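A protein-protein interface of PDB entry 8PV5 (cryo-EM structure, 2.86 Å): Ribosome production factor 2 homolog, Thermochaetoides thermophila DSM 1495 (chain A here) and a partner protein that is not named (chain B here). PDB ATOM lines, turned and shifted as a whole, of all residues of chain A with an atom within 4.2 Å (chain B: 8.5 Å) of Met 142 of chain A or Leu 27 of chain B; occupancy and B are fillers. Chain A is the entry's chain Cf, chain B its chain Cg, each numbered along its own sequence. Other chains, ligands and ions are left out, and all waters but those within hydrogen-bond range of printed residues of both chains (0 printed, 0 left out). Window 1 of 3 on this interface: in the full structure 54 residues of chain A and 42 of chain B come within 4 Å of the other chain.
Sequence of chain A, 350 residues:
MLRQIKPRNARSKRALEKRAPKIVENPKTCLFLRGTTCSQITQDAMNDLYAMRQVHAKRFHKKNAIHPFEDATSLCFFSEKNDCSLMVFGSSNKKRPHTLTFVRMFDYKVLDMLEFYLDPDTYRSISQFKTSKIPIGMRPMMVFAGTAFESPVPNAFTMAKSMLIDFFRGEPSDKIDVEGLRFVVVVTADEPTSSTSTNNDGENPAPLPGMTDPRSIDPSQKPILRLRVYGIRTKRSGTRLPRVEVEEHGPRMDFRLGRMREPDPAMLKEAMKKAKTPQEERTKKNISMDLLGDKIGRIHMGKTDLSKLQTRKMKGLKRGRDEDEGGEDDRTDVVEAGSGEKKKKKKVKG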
ATOM      1  N   ARG A 139      26.684   5.972  11.453  1.00  0.00           N
ATOM      2  CA  ARG A 139      25.934   4.962  10.722  1.00  0.00           C
ATOM      3  C   ARG A 139      26.627   3.604  10.840  1.00  0.00           C
ATOM      4  O   ARG A 139      27.839   3.501  10.633  1.00  0.00           O
ATOM      5  CB  ARG A 139      25.775   5.361   9.249  1.00  0.00           C
ATOM      6  CG  ARG A 139      27.065   5.757   8.546  1.00  0.00           C
ATOM      7  CD  ARG A 139      26.844   6.112   7.086  1.00  0.00           C
ATOM      8  NE  ARG A 139      26.498   4.947   6.280  1.00  0.00           N
ATOM      9  CZ  ARG A 139      26.148   5.000   5.003  1.00  0.00           C
ATOM     10  NH1 ARG A 139      26.108   6.145   4.344  1.00  0.00           N
ATOM     11  NH2 ARG A 139      25.839   3.873   4.368  1.00  0.00           N
ATOM     12  N   PRO A 140      25.899   2.560  11.212  1.00  0.00           N
ATOM     13  CA  PRO A 140      26.487   1.223  11.273  1.00  0.00           C
ATOM     14  C   PRO A 140      26.419   0.531   9.916  1.00  0.00           C
ATOM     15  O   PRO A 140      25.552   0.808   9.085  1.00  0.00           O
ATOM     16  CB  PRO A 140      25.602   0.510  12.301  1.00  0.00           C
ATOM     17  CG  PRO A 140      24.262   1.132  12.104  1.00  0.00           C
ATOM     18  CD  PRO A 140      24.502   2.569  11.685  1.00  0.00           C
ATOM     19  N   MET A 141      27.362  -0.377   9.704  1.00  0.00           N
ATOM     20  CA  MET A 141      27.372  -1.143   8.469  1.00  0.00           C
ATOM     21  C   MET A 141      26.338  -2.259   8.563  1.00  0.00           C
ATOM     22  O   MET A 141      25.844  -2.573   9.643  1.00  0.00           O
ATOM     23  CB  MET A 141      28.770  -1.693   8.207  1.00  0.00           C
ATOM     24  CG  MET A 141      29.842  -0.670   8.540  1.00  0.00           C
ATOM     25  SD  MET A 141      31.518  -1.185   8.166  1.00  0.00           S
ATOM     26  CE  MET A 141      31.699  -2.553   9.295  1.00  0.00           C
ATOM     27  N   MET A 142      25.983  -2.838   7.420  1.00  0.00           N
ATOM     28  CA  MET A 142      24.922  -3.838   7.390  1.00  0.00           C
ATOM     29  C   MET A 142      25.395  -5.125   6.737  1.00  0.00           C
ATOM     30  O   MET A 142      26.136  -5.101   5.750  1.00  0.00           O
ATOM     31  CB  MET A 142      23.679  -3.324   6.654  1.00  0.00           C
ATOM     32  CG  MET A 142      22.808  -2.395   7.481  1.00  0.00           C
ATOM     33  SD  MET A 142      21.919  -1.191   6.480  1.00  0.00           S
ATOM     34  CE  MET A 142      23.251  -0.509   5.509  1.00  0.00           C
ATOM     35  N   VAL A 143      24.963  -6.249   7.305  1.00  0.00           N
ATOM     36  CA  VAL A 143      25.208  -7.580   6.757  1.00  0.00           C
ATOM     37  C   VAL A 143      23.890  -8.343   6.773  1.00  0.00           C
ATOM     38  O   VAL A 143      23.287  -8.526   7.839  1.00  0.00           O
ATOM     39  CB  VAL A 143      26.285  -8.345   7.545  1.00  0.00           C
ATOM     40  CG1 VAL A 143      26.304  -9.808   7.137  1.00  0.00           C
ATOM     41  CG2 VAL A 143      27.653  -7.722   7.326  1.00  0.00           C
ATOM     42  N   PHE A 144      23.448  -8.791   5.602  1.00  0.00           N
ATOM     43  CA  PHE A 144      22.225  -9.574   5.459  1.00  0.00           C
ATOM     44  C   PHE A 144      22.622 -10.996   5.082  1.00  0.00           C
ATOM     45  O   PHE A 144      23.302 -11.209   4.073  1.00  0.00           O
ATOM     46  CB  PHE A 144      21.300  -8.957   4.412  1.00  0.00           C
ATOM     47  CG  PHE A 144      20.562  -7.746   4.898  1.00  0.00           C
ATOM     48  CD1 PHE A 144      21.179  -6.506   4.927  1.00  0.00           C
ATOM     49  CD2 PHE A 144      19.250  -7.845   5.330  1.00  0.00           C
ATOM     50  CE1 PHE A 144      20.503  -5.390   5.376  1.00  0.00           C
ATOM     51  CE2 PHE A 144      18.568  -6.731   5.780  1.00  0.00           C
ATOM     52  CZ  PHE A 144      19.195  -5.503   5.803  1.00  0.00           C
ATOM     53  N   ILE A 165      17.233  -1.910   5.267  1.00  0.00           N
ATOM     54  CA  ILE A 165      18.264  -1.132   4.584  1.00  0.00           C
ATOM     55  C   ILE A 165      17.935   0.352   4.649  1.00  0.00           C
ATOM     56  O   ILE A 165      18.796   1.182   4.966  1.00  0.00           O
ATOM     57  CB  ILE A 165      18.419  -1.610   3.128  1.00  0.00           C
ATOM     58  CG1 ILE A 165      19.089  -2.980   3.075  1.00  0.00           C
ATOM     59  CG2 ILE A 165      19.230  -0.619   2.312  1.00  0.00           C
ATOM     60  CD1 ILE A 165      18.956  -3.654   1.726  1.00  0.00           C
ATOM     61  N   PHE A 168      18.452   1.516   8.553  1.00  0.00           N
ATOM     62  CA  PHE A 168      19.840   1.656   8.973  1.00  0.00           C
ATOM     63  C   PHE A 168      20.730   2.232   7.878  1.00  0.00           C
ATOM     64  O   PHE A 168      21.953   2.068   7.937  1.00  0.00           O
ATOM     65  CB  PHE A 168      20.391   0.308   9.438  1.00  0.00           C
ATOM     66  CG  PHE A 168      19.712  -0.236  10.660  1.00  0.00           C
ATOM     67  CD1 PHE A 168      19.926   0.339  11.901  1.00  0.00           C
ATOM     68  CD2 PHE A 168      18.868  -1.329  10.570  1.00  0.00           C
ATOM     69  CE1 PHE A 168      19.304  -0.162  13.029  1.00  0.00           C
ATOM     70  CE2 PHE A 168      18.245  -1.835  11.693  1.00  0.00           C
ATOM     71  CZ  PHE A 168      18.463  -1.250  12.924  1.00  0.00           C
ATOM     72  N   ARG A 169      20.138   2.883   6.873  1.00  0.00           N
ATOM     73  CA  ARG A 169      20.922   3.508   5.813  1.00  0.00           C
ATOM     74  C   ARG A 169      21.762   4.663   6.341  1.00  0.00           C
ATOM     75  O   ARG A 169      22.932   4.808   5.970  1.00  0.00           O
ATOM     76  CB  ARG A 169      19.985   3.988   4.705  1.00  0.00           C
ATOM     77  CG  ARG A 169      20.652   4.244   3.370  1.00  0.00           C
ATOM     78  CD  ARG A 169      19.741   5.070   2.473  1.00  0.00           C
ATOM     79  NE  ARG A 169      20.293   5.270   1.139  1.00  0.00           N
ATOM     80  CZ  ARG A 169      21.247   6.143   0.841  1.00  0.00           C
ATOM     81  NH1 ARG A 169      21.777   6.930   1.762  1.00  0.00           N
ATOM     82  NH2 ARG A 169      21.677   6.229  -0.414  1.00  0.00           N
ATOM     83  N   VAL A 185      25.424  -4.290  11.845  1.00  0.00           N
ATOM     84  CA  VAL A 185      24.067  -4.744  12.102  1.00  0.00           C
ATOM     85  C   VAL A 185      23.784  -5.902  11.160  1.00  0.00           C
ATOM     86  O   VAL A 185      23.854  -5.746   9.935  1.00  0.00           O
ATOM     87  CB  VAL A 185      23.055  -3.605  11.900  1.00  0.00           C
ATOM     88  CG1 VAL A 185      21.645  -4.119  12.051  1.00  0.00           C
ATOM     89  CG2 VAL A 185      23.323  -2.478  12.884  1.00  0.00           C
ATOM     90  N   THR B  22      28.220 -10.825  -1.931  1.00  0.00           N
ATOM     91  CA  THR B  22      28.073  -9.669  -2.804  1.00  0.00           C
ATOM     92  C   THR B  22      28.104  -8.400  -1.963  1.00  0.00           C
ATOM     93  O   THR B  22      27.738  -8.403  -0.786  1.00  0.00           O
ATOM     94  CB  THR B  22      26.783  -9.737  -3.629  1.00  0.00           C
ATOM     95  OG1 THR B  22      25.651  -9.747  -2.757  1.00  0.00           O
ATOM     96  CG2 THR B  22      26.762 -10.989  -4.494  1.00  0.00           C
ATOM     97  N   PHE B  23      28.561  -7.308  -2.570  1.00  0.00           N
ATOM     98  CA  PHE B  23      28.849  -6.103  -1.811  1.00  0.00           C
ATOM     99  C   PHE B  23      28.209  -4.887  -2.459  1.00  0.00           C
ATOM    100  O   PHE B  23      28.037  -4.823  -3.679  1.00  0.00           O
ATOM    101  CB  PHE B  23      30.360  -5.879  -1.674  1.00  0.00           C
ATOM    102  CG  PHE B  23      31.046  -6.911  -0.832  1.00  0.00           C
ATOM    103  CD1 PHE B  23      31.028  -6.819   0.548  1.00  0.00           C
ATOM    104  CD2 PHE B  23      31.707  -7.975  -1.419  1.00  0.00           C
ATOM    105  CE1 PHE B  23      31.657  -7.771   1.327  1.00  0.00           C
ATOM    106  CE2 PHE B  23      32.338  -8.929  -0.646  1.00  0.00           C
ATOM    107  CZ  PHE B  23      32.313  -8.826   0.728  1.00  0.00           C
ATOM    108  N   ASP B  24      27.852  -3.915  -1.609  1.00  0.00           N
ATOM    109  CA  ASP B  24      27.400  -2.584  -2.013  1.00  0.00           C
ATOM    110  C   ASP B  24      28.099  -1.618  -1.057  1.00  0.00           C
ATOM    111  O   ASP B  24      27.615  -1.326   0.037  1.00  0.00           O
ATOM    112  CB  ASP B  24      25.879  -2.453  -1.954  1.00  0.00           C
ATOM    113  CG  ASP B  24      25.393  -1.083  -2.379  1.00  0.00           C
ATOM    114  OD1 ASP B  24      26.144  -0.364  -3.071  1.00  0.00           O
ATOM    115  OD2 ASP B  24      24.256  -0.721  -2.015  1.00  0.00           O
ATOM    116  N   LEU B  25      29.270  -1.135  -1.467  1.00  0.00           N
ATOM    117  CA  LEU B  25      30.084  -0.337  -0.560  1.00  0.00           C
ATOM    118  C   LEU B  25      29.608   1.105  -0.470  1.00  0.00           C
ATOM    119  O   LEU B  25      30.111   1.859   0.368  1.00  0.00           O
ATOM    120  CB  LEU B  25      31.549  -0.400  -0.985  1.00  0.00           C
ATOM    121  CG  LEU B  25      32.129  -1.816  -0.956  1.00  0.00           C
ATOM    122  CD1 LEU B  25      33.614  -1.790  -1.237  1.00  0.00           C
ATOM    123  CD2 LEU B  25      31.849  -2.495   0.378  1.00  0.00           C
ATOM    124  N   GLY B  26      28.658   1.507  -1.315  1.00  0.00           N
ATOM    125  CA  GLY B  26      28.029   2.803  -1.137  1.00  0.00           C
ATOM    126  C   GLY B  26      27.195   2.881   0.125  1.00  0.00           C
ATOM    127  O   GLY B  26      27.168   3.917   0.794  1.00  0.00           O
ATOM    128  N   LEU B  27      26.508   1.792   0.467  1.00  0.00           N
ATOM    129  CA  LEU B  27      25.721   1.708   1.689  1.00  0.00           C
ATOM    130  C   LEU B  27      26.406   0.886   2.772  1.00  0.00           C
ATOM    131  O   LEU B  27      25.795   0.642   3.817  1.00  0.00           O
ATOM    132  CB  LEU B  27      24.341   1.121   1.392  1.00  0.00           C
ATOM    133  CG  LEU B  27      23.508   1.850   0.341  1.00  0.00           C
ATOM    134  CD1 LEU B  27      22.159   1.178   0.173  1.00  0.00           C
ATOM    135  CD2 LEU B  27      23.340   3.305   0.731  1.00  0.00           C
ATOM    136  N   LEU B  28      27.659   0.472   2.544  1.00  0.00           N
ATOM    137  CA  LEU B  28      28.420  -0.392   3.458  1.00  0.00           C
ATOM    138  C   LEU B  28      27.659  -1.679   3.759  1.00  0.00           C
ATOM    139  O   LEU B  28      27.446  -2.045   4.916  1.00  0.00           O
ATOM    140  CB  LEU B  28      28.780   0.342   4.751  1.00  0.00           C
ATOM    141  CG  LEU B  28      29.342   1.754   4.616  1.00  0.00           C
ATOM    142  CD1 LEU B  28      29.286   2.452   5.960  1.00  0.00           C
ATOM    143  CD2 LEU B  28      30.763   1.716   4.086  1.00  0.00           C
ATOM    144  N   LEU B  29      27.241  -2.372   2.705  1.00  0.00           N
ATOM    145  CA  LEU B  29      26.309  -3.482   2.814  1.00  0.00           C
ATOM    146  C   LEU B  29      26.929  -4.738   2.220  1.00  0.00           C
ATOM    147  O   LEU B  29      27.581  -4.679   1.172  1.00  0.00           O
ATOM    148  CB  LEU B  29      24.999  -3.128   2.106  1.00  0.00           C
ATOM    149  CG  LEU B  29      23.752  -4.002   2.189  1.00  0.00           C
ATOM    150  CD1 LEU B  29      22.578  -3.087   2.017  1.00  0.00           C
ATOM    151  CD2 LEU B  29      23.714  -5.067   1.110  1.00  0.00           C
ATOM    152  N   ALA B  30      26.716  -5.868   2.886  1.00  0.00           N
ATOM    153  CA  ALA B  30      27.154  -7.169   2.402  1.00  0.00           C
ATOM    154  C   ALA B  30      25.970  -8.123   2.397  1.00  0.00           C
ATOM    155  O   ALA B  30      25.245  -8.225   3.392  1.00  0.00           O
ATOM    156  CB  ALA B  30      28.283  -7.732   3.268  1.00  0.00           C
ATOM    157  N   ASN B  31      25.776  -8.818   1.279  1.00  0.00           N
ATOM    158  CA  ASN B  31      24.737  -9.831   1.146  1.00  0.00           C
ATOM    159  C   ASN B  31      25.416 -11.193   1.100  1.00  0.00           C
ATOM    160  O   ASN B  31      26.291 -11.433   0.255  1.00  0.00           O
ATOM    161  CB  ASN B  31      23.883  -9.595  -0.097  1.00  0.00           C
ATOM    162  CG  ASN B  31      23.002  -8.373   0.027  1.00  0.00           C
ATOM    163  OD1 ASN B  31      22.398  -8.135   1.071  1.00  0.00           O
ATOM    164  ND2 ASN B  31      22.926  -7.589  -1.041  1.00  0.00           N
ATOM    165  N   ASP B  32      25.013 -12.072   2.016  1.00  0.00           N
ATOM    166  CA  ASP B  32      25.579 -13.403   2.134  1.00  0.00           C
ATOM    167  C   ASP B  32      24.472 -14.361   1.720  1.00  0.00           C
ATOM    168  O   ASP B  32      23.565 -14.626   2.524  1.00  0.00           O
ATOM    169  CB  ASP B  32      26.025 -13.659   3.581  1.00  0.00           C
ATOM    170  CG  ASP B  32      26.467 -15.110   3.870  1.00  0.00           C
ATOM    171  OD1 ASP B  32      26.434 -16.011   3.005  1.00  0.00           O
ATOM    172  OD2 ASP B  32      26.862 -15.353   5.029  1.00  0.00           O
ATOM    173  N   ALA B  55      28.209 -13.382  11.728  1.00  0.00           N
ATOM    174  CA  ALA B  55      28.426 -11.938  11.737  1.00  0.00           C
ATOM    175  C   ALA B  55      29.902 -11.592  11.596  1.00  0.00           C
ATOM    176  O   ALA B  55      30.257 -10.622  10.917  1.00  0.00           O
ATOM    177  CB  ALA B  55      27.866 -11.338  13.022  1.00  0.00           C
ATOM    178  N   GLY B  58      30.917 -12.105   7.958  1.00  0.00           N
ATOM    179  CA  GLY B  58      30.426 -11.015   7.128  1.00  0.00           C
ATOM    180  C   GLY B  58      31.181  -9.717   7.345  1.00  0.00           C
ATOM    181  O   GLY B  58      31.540  -9.026   6.386  1.00  0.00           O
ATOM    182  N   ALA B  59      31.456  -9.380   8.609  1.00  0.00           N
ATOM    183  CA  ALA B  59      32.231  -8.182   8.911  1.00  0.00           C
ATOM    184  C   ALA B  59      33.652  -8.296   8.380  1.00  0.00           C
ATOM    185  O   ALA B  59      34.207  -7.317   7.870  1.00  0.00           O
ATOM    186  CB  ALA B  59      32.239  -7.927  10.417  1.00  0.00           C
ATOM    187  N   LEU B  62      33.618  -7.840   4.647  1.00  0.00           N
ATOM    188  CA  LEU B  62      33.241  -6.471   4.308  1.00  0.00           C
ATOM    189  C   LEU B  62      34.409  -5.509   4.528  1.00  0.00           C
ATOM    190  O   LEU B  62      34.678  -4.641   3.687  1.00  0.00           O
ATOM    191  CB  LEU B  62      32.006  -6.071   5.122  1.00  0.00           C
ATOM    192  CG  LEU B  62      31.222  -4.784   4.842  1.00  0.00           C
ATOM    193  CD1 LEU B  62      29.782  -4.977   5.267  1.00  0.00           C
ATOM    194  CD2 LEU B  62      31.792  -3.600   5.569  1.00  0.00           C
ATOM    195  N   LEU B  66      36.446  -3.351   1.712  1.00  0.00           N
ATOM    196  CA  LEU B  66      36.668  -1.913   1.860  1.00  0.00           C
ATOM    197  C   LEU B  66      38.149  -1.561   1.794  1.00  0.00           C
ATOM    198  O   LEU B  66      38.526  -0.563   1.171  1.00  0.00           O
ATOM    199  CB  LEU B  66      36.071  -1.411   3.174  1.00  0.00           C
ATOM    200  CG  LEU B  66      34.560  -1.219   3.249  1.00  0.00           C
ATOM    201  CD1 LEU B  66      34.155  -0.939   4.678  1.00  0.00           C
ATOM    202  CD2 LEU B  66      34.127  -0.085   2.340  1.00  0.00           C
ATOM    203  N   LEU B  83      34.083   5.912  -1.397  1.00  0.00           N
ATOM    204  CA  LEU B  83      33.032   4.932  -1.624  1.00  0.00           C
ATOM    205  C   LEU B  83      32.358   5.158  -2.970  1.00  0.00           C
ATOM    206  O   LEU B  83      32.181   6.306  -3.394  1.00  0.00           O
ATOM    207  CB  LEU B  83      31.979   5.003  -0.519  1.00  0.00           C
ATOM    208  CG  LEU B  83      32.466   4.815   0.917  1.00  0.00           C
ATOM    209  CD1 LEU B  83      31.352   5.132   1.897  1.00  0.00           C
ATOM    210  CD2 LEU B  83      32.994   3.407   1.132  1.00  0.00           C
ATOM    211  N   PRO B  84      31.981   4.074  -3.654  1.00  0.00           N
ATOM    212  CA  PRO B  84      31.207   4.221  -4.883  1.00  0.00           C
ATOM    213  C   PRO B  84      29.802   4.719  -4.572  1.00  0.00           C
ATOM    214  O   PRO B  84      29.364   4.681  -3.413  1.00  0.00           O
ATOM    215  CB  PRO B  84      31.178   2.793  -5.457  1.00  0.00           C
ATOM    216  CG  PRO B  84      31.492   1.905  -4.305  1.00  0.00           C
ATOM    217  CD  PRO B  84      32.413   2.685  -3.433  1.00  0.00           C
ATOM    218  N   PRO B  85      29.083   5.225  -5.571  1.00  0.00           N
ATOM    219  CA  PRO B  85      27.662   5.544  -5.369  1.00  0.00           C
ATOM    220  C   PRO B  85      26.863   4.288  -5.072  1.00  0.00           C
ATOM    221  O   PRO B  85      27.224   3.194  -5.533  1.00  0.00           O
ATOM    222  CB  PRO B  85      27.244   6.171  -6.708  1.00  0.00           C
ATOM    223  CG  PRO B  85      28.295   5.744  -7.683  1.00  0.00           C
ATOM    224  CD  PRO B  85      29.557   5.677  -6.889  1.00  0.00           C
ATOM    225  N   PRO B  86      25.794   4.398  -4.279  1.00  0.00           N
ATOM    226  CA  PRO B  86      25.005   3.209  -3.927  1.00  0.00           C
ATOM    227  C   PRO B  86      24.319   2.595  -5.140  1.00  0.00           C
ATOM    228  O   PRO B  86      23.898   3.295  -6.061  1.00  0.00           O
ATOM    229  CB  PRO B  86      23.982   3.748  -2.921  1.00  0.00           C
ATOM    230  CG  PRO B  86      24.574   5.018  -2.406  1.00  0.00           C
ATOM    231  CD  PRO B  86      25.344   5.595  -3.550  1.00  0.00           C
ATOM    232  N   THR B  87      24.211   1.267  -5.126  1.00  0.00           N
ATOM    233  CA  THR B  87      23.611   0.518  -6.222  1.00  0.00           C
ATOM    234  C   THR B  87      22.350  -0.233  -5.830  1.00  0.00           C
ATOM    235  O   THR B  87      21.604  -0.659  -6.716  1.00  0.00           O
ATOM    236  CB  THR B  87      24.617  -0.485  -6.802  1.00  0.00           C
ATOM    237  OG1 THR B  87      25.005  -1.418  -5.786  1.00  0.00           O
ATOM    238  CG2 THR B  87      25.852   0.234  -7.321  1.00  0.00           C
ATOM    239  N   THR B  88      22.099  -0.416  -4.541  1.00  0.00           N
ATOM    240  CA  THR B  88      20.890  -1.091  -4.092  1.00  0.00           C
ATOM    241  C   THR B  88      19.683  -0.189  -4.325  1.00  0.00           C
ATOM    242  O   THR B  88      19.674   0.955  -3.846  1.00  0.00           O
ATOM    243  CB  THR B  88      20.994  -1.457  -2.613  1.00  0.00           C
ATOM    244  OG1 THR B  88      22.059  -2.397  -2.425  1.00  0.00           O
ATOM    245  CG2 THR B  88      19.692  -2.071  -2.124  1.00  0.00           C
ATOM    246  N   PRO B  89      18.663  -0.646  -5.053  1.00  0.00           N
ATOM    247  CA  PRO B  89      17.503   0.216  -5.320  1.00  0.00           C
ATOM    248  C   PRO B  89      16.658   0.407  -4.070  1.00  0.00           C
ATOM    249  O   PRO B  89      16.263  -0.559  -3.413  1.00  0.00           O
ATOM    250  CB  PRO B  89      16.734  -0.547  -6.408  1.00  0.00           C
ATOM    251  CG  PRO B  89      17.701  -1.565  -6.939  1.00  0.00           C
ATOM    252  CD  PRO B  89      18.582  -1.916  -5.788  1.00  0.00           C
ATOM    253  N   LEU B  90      16.382   1.666  -3.747  1.00  0.00           N
ATOM    254  CA  LEU B  90      15.544   2.033  -2.618  1.00  0.00           C
ATOM    255  C   LEU B  90      14.528   3.063  -3.081  1.00  0.00           C
ATOM    256  O   LEU B  90      14.848   3.926  -3.907  1.00  0.00           O
ATOM    257  CB  LEU B  90      16.372   2.602  -1.456  1.00  0.00           C
ATOM    258  CG  LEU B  90      17.228   1.604  -0.677  1.00  0.00           C
ATOM    259  CD1 LEU B  90      18.251   2.331   0.179  1.00  0.00           C
ATOM    260  CD2 LEU B  90      16.353   0.705   0.176  1.00  0.00           C
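The backbone carbonyl oxygen of Ala 30 of chain B lies within hydrogen-bond range of the backbone NH of Phe 144 of chain A (2.9 Å). The backbone carbonyl oxygen of Met 142 of chain A is in hydrogen-bond range of the backbone NH of Ala 30 of chain B. N of Met 142 of chain A sits at hydrogen-bond distance from O of Leu 28 of chain B (3.0 Å). O of Leu 27 of chain B sits at hydrogen-bond distance from NH2 of Arg 139 of chain A (3.3 Å). The backbone NH (N) of Asp 32 of chain B is in hydrogen-bond range of the backbone carbonyl oxygen (O) of Phe 144 of chain A (2.8 Å).
The backbone carbonyl oxygen (O) of Thr 22 of chain B lies within hydrogen-bond range of the backbone NH (N) of Asn 31 of chain B. The backbone carbonyl oxygen (O) of Met 141 of chain A sits at hydrogen-bond distance from the backbone NH (N) of Val 185 of chain A, at 2.8 Å. NH2 of Arg 139 of chain A lies close to O of Arg 169 of chain A, at 3.4 Å. The backbone NH (N) of Val 143 of chain A is in hydrogen-bond range of the backbone carbonyl oxygen (O) of Val 185 of chain A. The backbone carbonyl oxygen (O) of Asp 24 of chain B sits at hydrogen-bond distance from the backbone NH (N) of Leu 29 of chain B (2.9 Å).
Arg 139 of chain A touches Gly 26 of chain B. Leu 28 of chain B touches Arg 139 of chain A. Leu 62 of chain B touches Met 141 of chain A (CD2 to SD, 3.6 Å). Met 142 of chain A touches Leu 29 of chain B (O to CA, 3.4 Å). Met 142 of chain A touches Leu 62 of chain B. Ala 30 of chain B touches Val 143 of chain A. Phe 144 of chain A touches Asn 31 of chain B. CD1 of Leu 29 of chain B touches CG1 of Ile 165 of chain A (3.6 Å). Leu 90 of chain B touches Ile 165 of chain A. Leu 90 of chain B touches Arg 169 of chain A (CD1 to NE, 3.7 Å).
Of chain B, only Leu 27, Leu 28, Leu 29, Ala 30 and Leu 62 come within 4 Å of Met 142 of chain A. Leu 27 of chain B touches three residues of chain A. Printed residues of chain B within 4 Å of Met 141 of chain A: Leu 28 and Leu 62. Of the printed residues of chain A, Ala 30 of chain B touches Met 142 (3.0 Å), Val 143 (3.4 Å) and Phe 144 (2.9 Å). Of the printed residues of chain A, Leu 28 of chain B touches Arg 139 (3.8 Å), Met 141 (3.6 Å) and Met 142 (3.0 Å). Of the printed residues of chain B, Arg 169 of chain A touches Leu 27, Pro 86 and Leu 90. Val 185 of chain A touches none of the printed residues of chain B. The nearest printed residue of chain A that does not touch Asn 31 of chain B is Val 143 of chain A (5.6 Å).
Hydrophobic or aromatic side chains of chain A that line the printed part of chain B: Met 141, Met 142, Phe 144 and Ile 165. Hydrophobic or aromatic side chains of chain B that line the printed part of chain A: Leu 27, Leu 28, Leu 29, Leu 62, Pro 86 and Leu 90. Among the printed residues, 19 pairs touch across the chains. Among the printed residues, no Asp or Glu carboxylate lies within 4 Å of a Lys or Arg side-chain nitrogen of the other chain.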
